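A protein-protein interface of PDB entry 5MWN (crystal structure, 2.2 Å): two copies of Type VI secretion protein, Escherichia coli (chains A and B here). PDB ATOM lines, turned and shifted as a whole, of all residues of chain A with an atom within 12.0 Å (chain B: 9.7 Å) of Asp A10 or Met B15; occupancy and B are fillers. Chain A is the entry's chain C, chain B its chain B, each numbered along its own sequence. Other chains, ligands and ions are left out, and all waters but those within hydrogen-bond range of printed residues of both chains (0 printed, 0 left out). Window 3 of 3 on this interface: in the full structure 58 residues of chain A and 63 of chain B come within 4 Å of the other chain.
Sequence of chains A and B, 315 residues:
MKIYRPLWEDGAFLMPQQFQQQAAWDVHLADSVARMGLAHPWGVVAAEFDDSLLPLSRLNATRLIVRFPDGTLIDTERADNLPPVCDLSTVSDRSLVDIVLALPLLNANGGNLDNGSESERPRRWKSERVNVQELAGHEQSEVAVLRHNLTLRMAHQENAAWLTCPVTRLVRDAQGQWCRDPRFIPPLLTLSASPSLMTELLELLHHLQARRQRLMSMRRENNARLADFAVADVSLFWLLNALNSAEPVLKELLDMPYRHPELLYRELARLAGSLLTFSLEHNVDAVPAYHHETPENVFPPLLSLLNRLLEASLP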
ATOM      1  N   PRO A   6      13.194   5.764 -11.325  1.00  0.00           N
ATOM      2  CA  PRO A   6      13.725   7.003 -11.936  1.00  0.00           C
ATOM      3  C   PRO A   6      12.773   8.196 -11.877  1.00  0.00           C
ATOM      4  O   PRO A   6      11.553   8.042 -11.969  1.00  0.00           O
ATOM      5  CB  PRO A   6      13.995   6.585 -13.385  1.00  0.00           C
ATOM      6  CG  PRO A   6      12.979   5.506 -13.643  1.00  0.00           C
ATOM      7  CD  PRO A   6      12.772   4.781 -12.349  1.00  0.00           C
ATOM      8  N   LEU A   7      13.343   9.389 -11.741  1.00  0.00           N
ATOM      9  CA  LEU A   7      12.608  10.645 -11.786  1.00  0.00           C
ATOM     10  C   LEU A   7      12.857  11.182 -13.202  1.00  0.00           C
ATOM     11  O   LEU A   7      14.015  11.323 -13.618  1.00  0.00           O
ATOM     12  CB  LEU A   7      13.171  11.620 -10.743  1.00  0.00           C
ATOM     13  CG  LEU A   7      12.283  12.339  -9.705  1.00  0.00           C
ATOM     14  CD1 LEU A   7      12.722  13.761  -9.585  1.00  0.00           C
ATOM     15  CD2 LEU A   7      10.789  12.374 -10.054  1.00  0.00           C
ATOM     16  N   TRP A   8      11.780  11.414 -13.959  1.00  0.00           N
ATOM     17  CA  TRP A   8      11.874  11.887 -15.341  1.00  0.00           C
ATOM     18  C   TRP A   8      11.810  13.407 -15.372  1.00  0.00           C
ATOM     19  O   TRP A   8      10.844  14.002 -14.886  1.00  0.00           O
ATOM     20  CB  TRP A   8      10.795  11.229 -16.214  1.00  0.00           C
ATOM     21  CG  TRP A   8      10.758   9.732 -16.093  1.00  0.00           C
ATOM     22  CD1 TRP A   8       9.927   8.997 -15.300  1.00  0.00           C
ATOM     23  CD2 TRP A   8      11.631   8.798 -16.738  1.00  0.00           C
ATOM     24  NE1 TRP A   8      10.194   7.651 -15.452  1.00  0.00           N
ATOM     25  CE2 TRP A   8      11.236   7.501 -16.329  1.00  0.00           C
ATOM     26  CE3 TRP A   8      12.674   8.926 -17.672  1.00  0.00           C
ATOM     27  CZ2 TRP A   8      11.836   6.342 -16.831  1.00  0.00           C
ATOM     28  CZ3 TRP A   8      13.288   7.777 -18.143  1.00  0.00           C
ATOM     29  CH2 TRP A   8      12.873   6.503 -17.718  1.00  0.00           C
ATOM     30  N   GLU A   9      12.877  14.035 -15.888  1.00  0.00           N
ATOM     31  CA  GLU A   9      13.011  15.495 -15.938  1.00  0.00           C
ATOM     32  C   GLU A   9      13.225  16.004 -17.349  1.00  0.00           C
ATOM     33  O   GLU A   9      13.886  15.332 -18.147  1.00  0.00           O
ATOM     34  CB  GLU A   9      14.196  15.959 -15.070  1.00  0.00           C
ATOM     35  CG  GLU A   9      14.046  15.689 -13.581  1.00  0.00           C
ATOM     36  CD  GLU A   9      15.303  15.883 -12.748  1.00  0.00           C
ATOM     37  OE1 GLU A   9      16.361  15.324 -13.118  1.00  0.00           O
ATOM     38  OE2 GLU A   9      15.211  16.555 -11.694  1.00  0.00           O
ATOM     39  N   ASP A  10      12.703  17.215 -17.651  1.00  0.00           N
ATOM     40  CA  ASP A  10      12.916  17.846 -18.954  1.00  0.00           C
ATOM     41  C   ASP A  10      14.316  18.423 -18.875  1.00  0.00           C
ATOM     42  O   ASP A  10      14.690  19.018 -17.858  1.00  0.00           O
ATOM     43  CB  ASP A  10      11.903  18.953 -19.258  1.00  0.00           C
ATOM     44  CG  ASP A  10      11.874  19.322 -20.736  1.00  0.00           C
ATOM     45  OD1 ASP A  10      12.620  20.244 -21.134  1.00  0.00           O
ATOM     46  OD2 ASP A  10      11.144  18.651 -21.502  1.00  0.00           O
ATOM     47  N   GLY A  11      15.107  18.152 -19.885  1.00  0.00           N
ATOM     48  CA  GLY A  11      16.487  18.611 -19.915  1.00  0.00           C
ATOM     49  C   GLY A  11      17.489  17.599 -19.381  1.00  0.00           C
ATOM     50  O   GLY A  11      18.674  17.916 -19.232  1.00  0.00           O
ATOM     51  N   ALA A  12      17.010  16.385 -19.047  1.00  0.00           N
ATOM     52  CA  ALA A  12      17.861  15.306 -18.557  1.00  0.00           C
ATOM     53  C   ALA A  12      18.355  14.420 -19.692  1.00  0.00           C
ATOM     54  O   ALA A  12      17.625  14.154 -20.650  1.00  0.00           O
ATOM     55  CB  ALA A  12      17.117  14.460 -17.538  1.00  0.00           C
ATOM     56  N   PHE A  13      19.590  13.947 -19.564  1.00  0.00           N
ATOM     57  CA  PHE A  13      20.227  13.011 -20.481  1.00  0.00           C
ATOM     58  C   PHE A  13      19.593  11.644 -20.185  1.00  0.00           C
ATOM     59  O   PHE A  13      19.608  11.234 -19.019  1.00  0.00           O
ATOM     60  CB  PHE A  13      21.732  12.919 -20.140  1.00  0.00           C
ATOM     61  CG  PHE A  13      22.644  14.019 -20.624  1.00  0.00           C
ATOM     62  CD1 PHE A  13      22.758  14.297 -21.975  1.00  0.00           C
ATOM     63  CD2 PHE A  13      23.522  14.658 -19.744  1.00  0.00           C
ATOM     64  CE1 PHE A  13      23.646  15.270 -22.430  1.00  0.00           C
ATOM     65  CE2 PHE A  13      24.409  15.641 -20.202  1.00  0.00           C
ATOM     66  CZ  PHE A  13      24.456  15.943 -21.542  1.00  0.00           C
ATOM     67  N   LEU A  14      19.031  10.942 -21.188  1.00  0.00           N
ATOM     68  CA  LEU A  14      18.445   9.621 -20.922  1.00  0.00           C
ATOM     69  C   LEU A  14      19.528   8.570 -20.779  1.00  0.00           C
ATOM     70  O   LEU A  14      20.442   8.505 -21.593  1.00  0.00           O
ATOM     71  CB  LEU A  14      17.358   9.225 -21.935  1.00  0.00           C
ATOM     72  CG  LEU A  14      16.093  10.096 -21.888  1.00  0.00           C
ATOM     73  CD1 LEU A  14      15.248   9.891 -23.102  1.00  0.00           C
ATOM     74  CD2 LEU A  14      15.248   9.802 -20.655  1.00  0.00           C
ATOM     75  N   MET A  15      19.467   7.815 -19.687  1.00  0.00           N
ATOM     76  CA  MET A  15      20.458   6.810 -19.331  1.00  0.00           C
ATOM     77  C   MET A  15      19.862   5.412 -19.287  1.00  0.00           C
ATOM     78  O   MET A  15      18.704   5.275 -18.878  1.00  0.00           O
ATOM     79  CB  MET A  15      21.076   7.156 -17.962  1.00  0.00           C
ATOM     80  CG  MET A  15      21.949   8.417 -17.984  1.00  0.00           C
ATOM     81  SD  MET A  15      23.347   8.356 -19.159  1.00  0.00           S
ATOM     82  CE  MET A  15      24.321   7.059 -18.425  1.00  0.00           C
ATOM     83  N   GLN A  18      17.931   4.332 -16.011  1.00  0.00           N
ATOM     84  CA  GLN A  18      16.553   4.793 -15.816  1.00  0.00           C
ATOM     85  C   GLN A  18      15.529   3.739 -16.291  1.00  0.00           C
ATOM     86  O   GLN A  18      14.598   3.402 -15.563  1.00  0.00           O
ATOM     87  CB  GLN A  18      16.317   6.125 -16.544  1.00  0.00           C
ATOM     88  CG  GLN A  18      17.095   7.302 -15.970  1.00  0.00           C
ATOM     89  CD  GLN A  18      16.878   8.518 -16.812  1.00  0.00           C
ATOM     90  OE1 GLN A  18      17.238   8.551 -17.988  1.00  0.00           O
ATOM     91  NE2 GLN A  18      16.248   9.536 -16.247  1.00  0.00           N
ATOM     92  N   PHE A  19      15.749   3.185 -17.485  1.00  0.00           N
ATOM     93  CA  PHE A  19      14.891   2.161 -18.069  1.00  0.00           C
ATOM     94  C   PHE A  19      15.078   0.796 -17.402  1.00  0.00           C
ATOM     95  O   PHE A  19      14.098   0.066 -17.245  1.00  0.00           O
ATOM     96  CB  PHE A  19      15.085   2.096 -19.595  1.00  0.00           C
ATOM     97  CG  PHE A  19      15.004   3.445 -20.269  1.00  0.00           C
ATOM     98  CD1 PHE A  19      13.783   4.092 -20.425  1.00  0.00           C
ATOM     99  CD2 PHE A  19      16.154   4.094 -20.711  1.00  0.00           C
ATOM    100  CE1 PHE A  19      13.715   5.363 -21.019  1.00  0.00           C
ATOM    101  CE2 PHE A  19      16.079   5.360 -21.318  1.00  0.00           C
ATOM    102  CZ  PHE A  19      14.862   5.982 -21.467  1.00  0.00           C
ATOM    103  N   GLN A  22      13.311   1.120 -13.839  1.00  0.00           N
ATOM    104  CA  GLN A  22      11.858   1.160 -14.025  1.00  0.00           C
ATOM    105  C   GLN A  22      11.335  -0.246 -14.318  1.00  0.00           C
ATOM    106  O   GLN A  22      10.382  -0.680 -13.682  1.00  0.00           O
ATOM    107  CB  GLN A  22      11.468   2.165 -15.135  1.00  0.00           C
ATOM    108  CG  GLN A  22       9.968   2.425 -15.272  1.00  0.00           C
ATOM    109  CD  GLN A  22       9.362   3.070 -14.058  1.00  0.00           C
ATOM    110  OE1 GLN A  22       8.712   2.404 -13.234  1.00  0.00           O
ATOM    111  NE2 GLN A  22       9.545   4.384 -13.943  1.00  0.00           N
ATOM    112  N   TYR B   4      -2.715   8.723 -19.411  1.00  0.00           N
ATOM    113  CA  TYR B   4      -2.551   8.883 -20.847  1.00  0.00           C
ATOM    114  C   TYR B   4      -1.473   7.974 -21.397  1.00  0.00           C
ATOM    115  O   TYR B   4      -0.337   8.426 -21.530  1.00  0.00           O
ATOM    116  CB  TYR B   4      -2.256  10.356 -21.195  1.00  0.00           C
ATOM    117  CG  TYR B   4      -3.293  11.331 -20.684  1.00  0.00           C
ATOM    118  CD1 TYR B   4      -4.440  11.609 -21.422  1.00  0.00           C
ATOM    119  CD2 TYR B   4      -3.121  11.990 -19.472  1.00  0.00           C
ATOM    120  CE1 TYR B   4      -5.402  12.502 -20.954  1.00  0.00           C
ATOM    121  CE2 TYR B   4      -4.073  12.886 -18.995  1.00  0.00           C
ATOM    122  CZ  TYR B   4      -5.209  13.147 -19.743  1.00  0.00           C
ATOM    123  OH  TYR B   4      -6.149  14.034 -19.279  1.00  0.00           O
ATOM    124  N   PRO B   6       1.210   6.406 -23.496  1.00  0.00           N
ATOM    125  CA  PRO B   6       1.928   7.060 -24.600  1.00  0.00           C
ATOM    126  C   PRO B   6       2.014   6.224 -25.874  1.00  0.00           C
ATOM    127  O   PRO B   6       2.122   4.989 -25.831  1.00  0.00           O
ATOM    128  CB  PRO B   6       3.326   7.310 -24.020  1.00  0.00           C
ATOM    129  CG  PRO B   6       3.506   6.215 -23.033  1.00  0.00           C
ATOM    130  CD  PRO B   6       2.143   5.909 -22.462  1.00  0.00           C
ATOM    131  N   LEU B   7       1.993   6.918 -27.010  1.00  0.00           N
ATOM    132  CA  LEU B   7       2.198   6.308 -28.306  1.00  0.00           C
ATOM    133  C   LEU B   7       3.638   6.642 -28.666  1.00  0.00           C
ATOM    134  O   LEU B   7       4.021   7.812 -28.624  1.00  0.00           O
ATOM    135  CB  LEU B   7       1.225   6.858 -29.357  1.00  0.00           C
ATOM    136  CG  LEU B   7       0.148   5.888 -29.814  1.00  0.00           C
ATOM    137  CD1 LEU B   7      -0.855   6.577 -30.633  1.00  0.00           C
ATOM    138  CD2 LEU B   7       0.718   4.681 -30.529  1.00  0.00           C
ATOM    139  N   TRP B   8       4.456   5.622 -28.933  1.00  0.00           N
ATOM    140  CA  TRP B   8       5.876   5.802 -29.262  1.00  0.00           C
ATOM    141  C   TRP B   8       6.050   5.924 -30.769  1.00  0.00           C
ATOM    142  O   TRP B   8       5.674   5.011 -31.505  1.00  0.00           O
ATOM    143  CB  TRP B   8       6.711   4.669 -28.647  1.00  0.00           C
ATOM    144  CG  TRP B   8       6.439   4.464 -27.180  1.00  0.00           C
ATOM    145  CD1 TRP B   8       5.597   3.553 -26.618  1.00  0.00           C
ATOM    146  CD2 TRP B   8       6.968   5.244 -26.098  1.00  0.00           C
ATOM    147  NE1 TRP B   8       5.605   3.682 -25.245  1.00  0.00           N
ATOM    148  CE2 TRP B   8       6.436   4.716 -24.900  1.00  0.00           C
ATOM    149  CE3 TRP B   8       7.890   6.303 -26.019  1.00  0.00           C
ATOM    150  CZ2 TRP B   8       6.806   5.201 -23.641  1.00  0.00           C
ATOM    151  CZ3 TRP B   8       8.230   6.800 -24.779  1.00  0.00           C
ATOM    152  CH2 TRP B   8       7.686   6.258 -23.607  1.00  0.00           C
ATOM    153  N   GLU B   9       6.556   7.082 -31.233  1.00  0.00           N
ATOM    154  CA  GLU B   9       6.686   7.406 -32.659  1.00  0.00           C
ATOM    155  C   GLU B   9       8.117   7.635 -33.087  1.00  0.00           C
ATOM    156  O   GLU B   9       8.901   8.157 -32.303  1.00  0.00           O
ATOM    157  CB  GLU B   9       5.854   8.650 -32.997  1.00  0.00           C
ATOM    158  CG  GLU B   9       4.353   8.454 -32.881  1.00  0.00           C
ATOM    159  CD  GLU B   9       3.533   9.727 -32.980  1.00  0.00           C
ATOM    160  OE1 GLU B   9       3.838  10.696 -32.246  1.00  0.00           O
ATOM    161  OE2 GLU B   9       2.557   9.741 -33.765  1.00  0.00           O
ATOM    162  N   ALA B  12       9.712  11.478 -32.931  1.00  0.00           N
ATOM    163  CA  ALA B  12       9.335  12.104 -31.674  1.00  0.00           C
ATOM    164  C   ALA B  12      10.442  12.423 -30.680  1.00  0.00           C
ATOM    165  O   ALA B  12      11.315  11.599 -30.400  1.00  0.00           O
ATOM    166  CB  ALA B  12       8.275  11.276 -30.990  1.00  0.00           C
ATOM    167  N   PHE B  13      10.364  13.646 -30.116  1.00  0.00           N
ATOM    168  CA  PHE B  13      11.262  14.102 -29.059  1.00  0.00           C
ATOM    169  C   PHE B  13      10.685  13.508 -27.772  1.00  0.00           C
ATOM    170  O   PHE B  13       9.478  13.591 -27.526  1.00  0.00           O
ATOM    171  CB  PHE B  13      11.315  15.631 -28.963  1.00  0.00           C
ATOM    172  CG  PHE B  13      11.807  16.439 -30.148  1.00  0.00           C
ATOM    173  CD1 PHE B  13      12.551  15.844 -31.167  1.00  0.00           C
ATOM    174  CD2 PHE B  13      11.529  17.790 -30.241  1.00  0.00           C
ATOM    175  CE1 PHE B  13      12.991  16.598 -32.264  1.00  0.00           C
ATOM    176  CE2 PHE B  13      11.998  18.545 -31.317  1.00  0.00           C
ATOM    177  CZ  PHE B  13      12.732  17.949 -32.318  1.00  0.00           C
ATOM    178  N   LEU B  14      11.526  12.830 -27.004  1.00  0.00           N
ATOM    179  CA  LEU B  14      11.097  12.157 -25.787  1.00  0.00           C
ATOM    180  C   LEU B  14      10.804  13.151 -24.682  1.00  0.00           C
ATOM    181  O   LEU B  14      11.593  14.067 -24.430  1.00  0.00           O
ATOM    182  CB  LEU B  14      12.083  11.049 -25.367  1.00  0.00           C
ATOM    183  CG  LEU B  14      12.157   9.856 -26.346  1.00  0.00           C
ATOM    184  CD1 LEU B  14      13.385   9.023 -26.119  1.00  0.00           C
ATOM    185  CD2 LEU B  14      10.909   8.989 -26.266  1.00  0.00           C
ATOM    186  N   MET B  15       9.617  13.005 -24.086  1.00  0.00           N
ATOM    187  CA  MET B  15       9.104  13.881 -23.038  1.00  0.00           C
ATOM    188  C   MET B  15       8.934  13.144 -21.718  1.00  0.00           C
ATOM    189  O   MET B  15       8.556  11.962 -21.735  1.00  0.00           O
ATOM    190  CB  MET B  15       7.769  14.495 -23.476  1.00  0.00           C
ATOM    191  CG  MET B  15       7.893  15.481 -24.640  1.00  0.00           C
ATOM    192  SD  MET B  15       9.014  16.896 -24.351  1.00  0.00           S
ATOM    193  CE  MET B  15       8.160  17.729 -23.044  1.00  0.00           C
ATOM    194  N   PRO B  16       9.160  13.822 -20.558  1.00  0.00           N
ATOM    195  CA  PRO B  16       8.977  13.135 -19.268  1.00  0.00           C
ATOM    196  C   PRO B  16       7.565  12.588 -19.057  1.00  0.00           C
ATOM    197  O   PRO B  16       7.434  11.517 -18.462  1.00  0.00           O
ATOM    198  CB  PRO B  16       9.392  14.183 -18.227  1.00  0.00           C
ATOM    199  CG  PRO B  16       9.329  15.475 -18.925  1.00  0.00           C
ATOM    200  CD  PRO B  16       9.607  15.217 -20.363  1.00  0.00           C
ATOM    201  N   GLN B  17       6.528  13.264 -19.611  1.00  0.00           N
ATOM    202  CA  GLN B  17       5.128  12.811 -19.510  1.00  0.00           C
ATOM    203  C   GLN B  17       4.914  11.416 -20.084  1.00  0.00           C
ATOM    204  O   GLN B  17       4.141  10.662 -19.508  1.00  0.00           O
ATOM    205  CB  GLN B  17       4.115  13.786 -20.142  1.00  0.00           C
ATOM    206  CG  GLN B  17       4.161  15.171 -19.576  1.00  0.00           C
ATOM    207  CD  GLN B  17       5.081  16.116 -20.294  1.00  0.00           C
ATOM    208  OE1 GLN B  17       6.293  15.966 -20.320  1.00  0.00           O
ATOM    209  NE2 GLN B  17       4.522  17.276 -20.556  1.00  0.00           N
ATOM    210  N   GLN B  18       5.631  11.044 -21.162  1.00  0.00           N
ATOM    211  CA  GLN B  18       5.529   9.715 -21.778  1.00  0.00           C
ATOM    212  C   GLN B  18       5.914   8.605 -20.794  1.00  0.00           C
ATOM    213  O   GLN B  18       5.173   7.634 -20.626  1.00  0.00           O
ATOM    214  CB  GLN B  18       6.401   9.637 -23.041  1.00  0.00           C
ATOM    215  CG  GLN B  18       5.929  10.514 -24.193  1.00  0.00           C
ATOM    216  CD  GLN B  18       6.908  10.450 -25.336  1.00  0.00           C
ATOM    217  OE1 GLN B  18       8.071  10.838 -25.222  1.00  0.00           O
ATOM    218  NE2 GLN B  18       6.463   9.906 -26.445  1.00  0.00           N
ATOM    219  N   PHE B  19       7.047   8.792 -20.097  1.00  0.00           N
ATOM    220  CA  PHE B  19       7.541   7.835 -19.106  1.00  0.00           C
ATOM    221  C   PHE B  19       6.732   7.856 -17.817  1.00  0.00           C
ATOM    222  O   PHE B  19       6.530   6.799 -17.213  1.00  0.00           O
ATOM    223  CB  PHE B  19       9.038   8.062 -18.848  1.00  0.00           C
ATOM    224  CG  PHE B  19       9.857   8.124 -20.118  1.00  0.00           C
ATOM    225  CD1 PHE B  19      10.127   6.973 -20.849  1.00  0.00           C
ATOM    226  CD2 PHE B  19      10.333   9.340 -20.598  1.00  0.00           C
ATOM    227  CE1 PHE B  19      10.858   7.032 -22.034  1.00  0.00           C
ATOM    228  CE2 PHE B  19      11.083   9.399 -21.777  1.00  0.00           C
ATOM    229  CZ  PHE B  19      11.341   8.243 -22.488  1.00  0.00           C
ATOM    230  N   GLN B  20       6.245   9.041 -17.408  1.00  0.00           N
ATOM    231  CA  GLN B  20       5.427   9.189 -16.196  1.00  0.00           C
ATOM    232  C   GLN B  20       4.085   8.494 -16.368  1.00  0.00           C
ATOM    233  O   GLN B  20       3.629   7.809 -15.458  1.00  0.00           O
ATOM    234  CB  GLN B  20       5.196  10.670 -15.846  1.00  0.00           C
ATOM    235  CG  GLN B  20       6.432  11.374 -15.300  1.00  0.00           C
ATOM    236  CD  GLN B  20       6.301  12.879 -15.282  1.00  0.00           C
ATOM    237  OE1 GLN B  20       5.286  13.464 -15.699  1.00  0.00           O
ATOM    238  NE2 GLN B  20       7.350  13.539 -14.798  1.00  0.00           N
ATOM    239  N   GLN B  21       3.463   8.670 -17.536  1.00  0.00           N
ATOM    240  CA  GLN B  21       2.160   8.084 -17.854  1.00  0.00           C
ATOM    241  C   GLN B  21       2.221   6.573 -18.006  1.00  0.00           C
ATOM    242  O   GLN B  21       1.335   5.880 -17.499  1.00  0.00           O
ATOM    243  CB  GLN B  21       1.543   8.753 -19.083  1.00  0.00           C
ATOM    244  CG  GLN B  21       1.112  10.212 -18.865  1.00  0.00           C
ATOM    245  CD  GLN B  21       0.180  10.419 -17.696  1.00  0.00           C
ATOM    246  OE1 GLN B  21       0.188  11.464 -17.049  1.00  0.00           O
ATOM    247  NE2 GLN B  21      -0.648   9.437 -17.407  1.00  0.00           N
ATOM    248  N   GLN B  22       3.273   6.063 -18.670  1.00  0.00           N
ATOM    249  CA  GLN B  22       3.491   4.628 -18.850  1.00  0.00           C
ATOM    250  C   GLN B  22       3.654   3.954 -17.486  1.00  0.00           C
ATOM    251  O   GLN B  22       2.992   2.942 -17.218  1.00  0.00           O
ATOM    252  CB  GLN B  22       4.706   4.361 -19.764  1.00  0.00           C
ATOM    253  CG  GLN B  22       4.889   2.889 -20.162  1.00  0.00           C
ATOM    254  CD  GLN B  22       3.740   2.342 -20.993  1.00  0.00           C
ATOM    255  OE1 GLN B  22       3.399   2.861 -22.058  1.00  0.00           O
ATOM    256  NE2 GLN B  22       3.103   1.291 -20.510  1.00  0.00           N
ATOM    257  N   ALA B 144      18.854  11.062 -11.205  1.00  0.00           N
ATOM    258  CA  ALA B 144      17.849  11.641 -10.305  1.00  0.00           C
ATOM    259  C   ALA B 144      16.873  10.511  -9.966  1.00  0.00           C
ATOM    260  O   ALA B 144      16.152  10.039 -10.845  1.00  0.00           O
ATOM    261  CB  ALA B 144      17.117  12.793 -10.992  1.00  0.00           C
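The backbone NH (N) of Met B15 is in hydrogen-bond range of the side-chain amide oxygen (OE1) of Gln B18.
Among the printed residues, merely in contact across the chains: Trp A8 with Phe B19 (3.4 Å), Glu A9 with Ala B144 (3.4 Å), Phe A19 with Phe B19 (3.5 Å), Asp A10 with Met B15 (3.5 Å), Trp A8 with Gln B20 (3.5 Å), Trp A8 with Pro B16 (3.6 Å), Leu A14 with Leu B14 (3.7 Å), Asp A10 with Pro B16 (3.9 Å) and Pro A6 with Ala B144 (3.98 Å).
Of the 17 printed residues of chain B, 6 touch a printed residue of chain A.
Hydrophobic or aromatic side chains of chain B that line the printed part of chain A: Leu B14, Met B15, Pro B16, Phe B19 and Ala B144.
Of the 13 printed residues of chain A, 7 touch a printed residue of chain B.
Printed residues of chain A that touch a printed residue of chain B: Pro A6, Leu A7, Trp A8, Glu A9, Asp A10, Leu A14 and Phe A19.
Hydrophobic or aromatic side chains of chain A that line the printed part of chain B: Leu A7, Trp A8, Leu A14 and Phe A19.
Along chain A the printed residues that touch a printed residue of chain B span positions 6 to 19.
Among the printed residues, 10 pairs touch across the chains.
Trp A8 touches Phe B19, but with the chains exchanged Phe A19 does not touch Trp B8 (6.6 Å).
Leu A14 touches its own counterpart, Leu B14.
Phe B19 touches its own counterpart, Phe A19.
Of chain B, only Met B15 (3.5 Å) and Pro B16 (3.9 Å) come within 4 Å of Asp A10.
No residue of chain B comes within 4 Å of Gly A11.
Pro B16 touches just these residues of chain A: Trp A8 and Asp A10.
Gln B17 touches none of the printed residues of chain A.
No residue of chain A comes within 4 Å of Gln B18.
Phe B19 touches just these residues of chain A: Trp A8 (3.4 Å) and Phe A19 (3.5 Å).
Of the printed residues of chain B, Leu A7 touches Ala B144.
Printed residues of chain B within 4 Å of Trp A8: Pro B16, Phe B19 and Gln B20.
Pro B6 touches none of the printed residues of chain A.
Ala B12 touches none of the printed residues of chain A.
The nearest residue of chain A that does not touch Met B15 is Trp A8 (6.0 Å).
The nearest printed residue of chain A that does not touch Ala B144 is Gln A18 (5.4 Å).
N of Leu A7 lies within hydrogen-bond range of O of Ala B144, at 3.0 Å.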
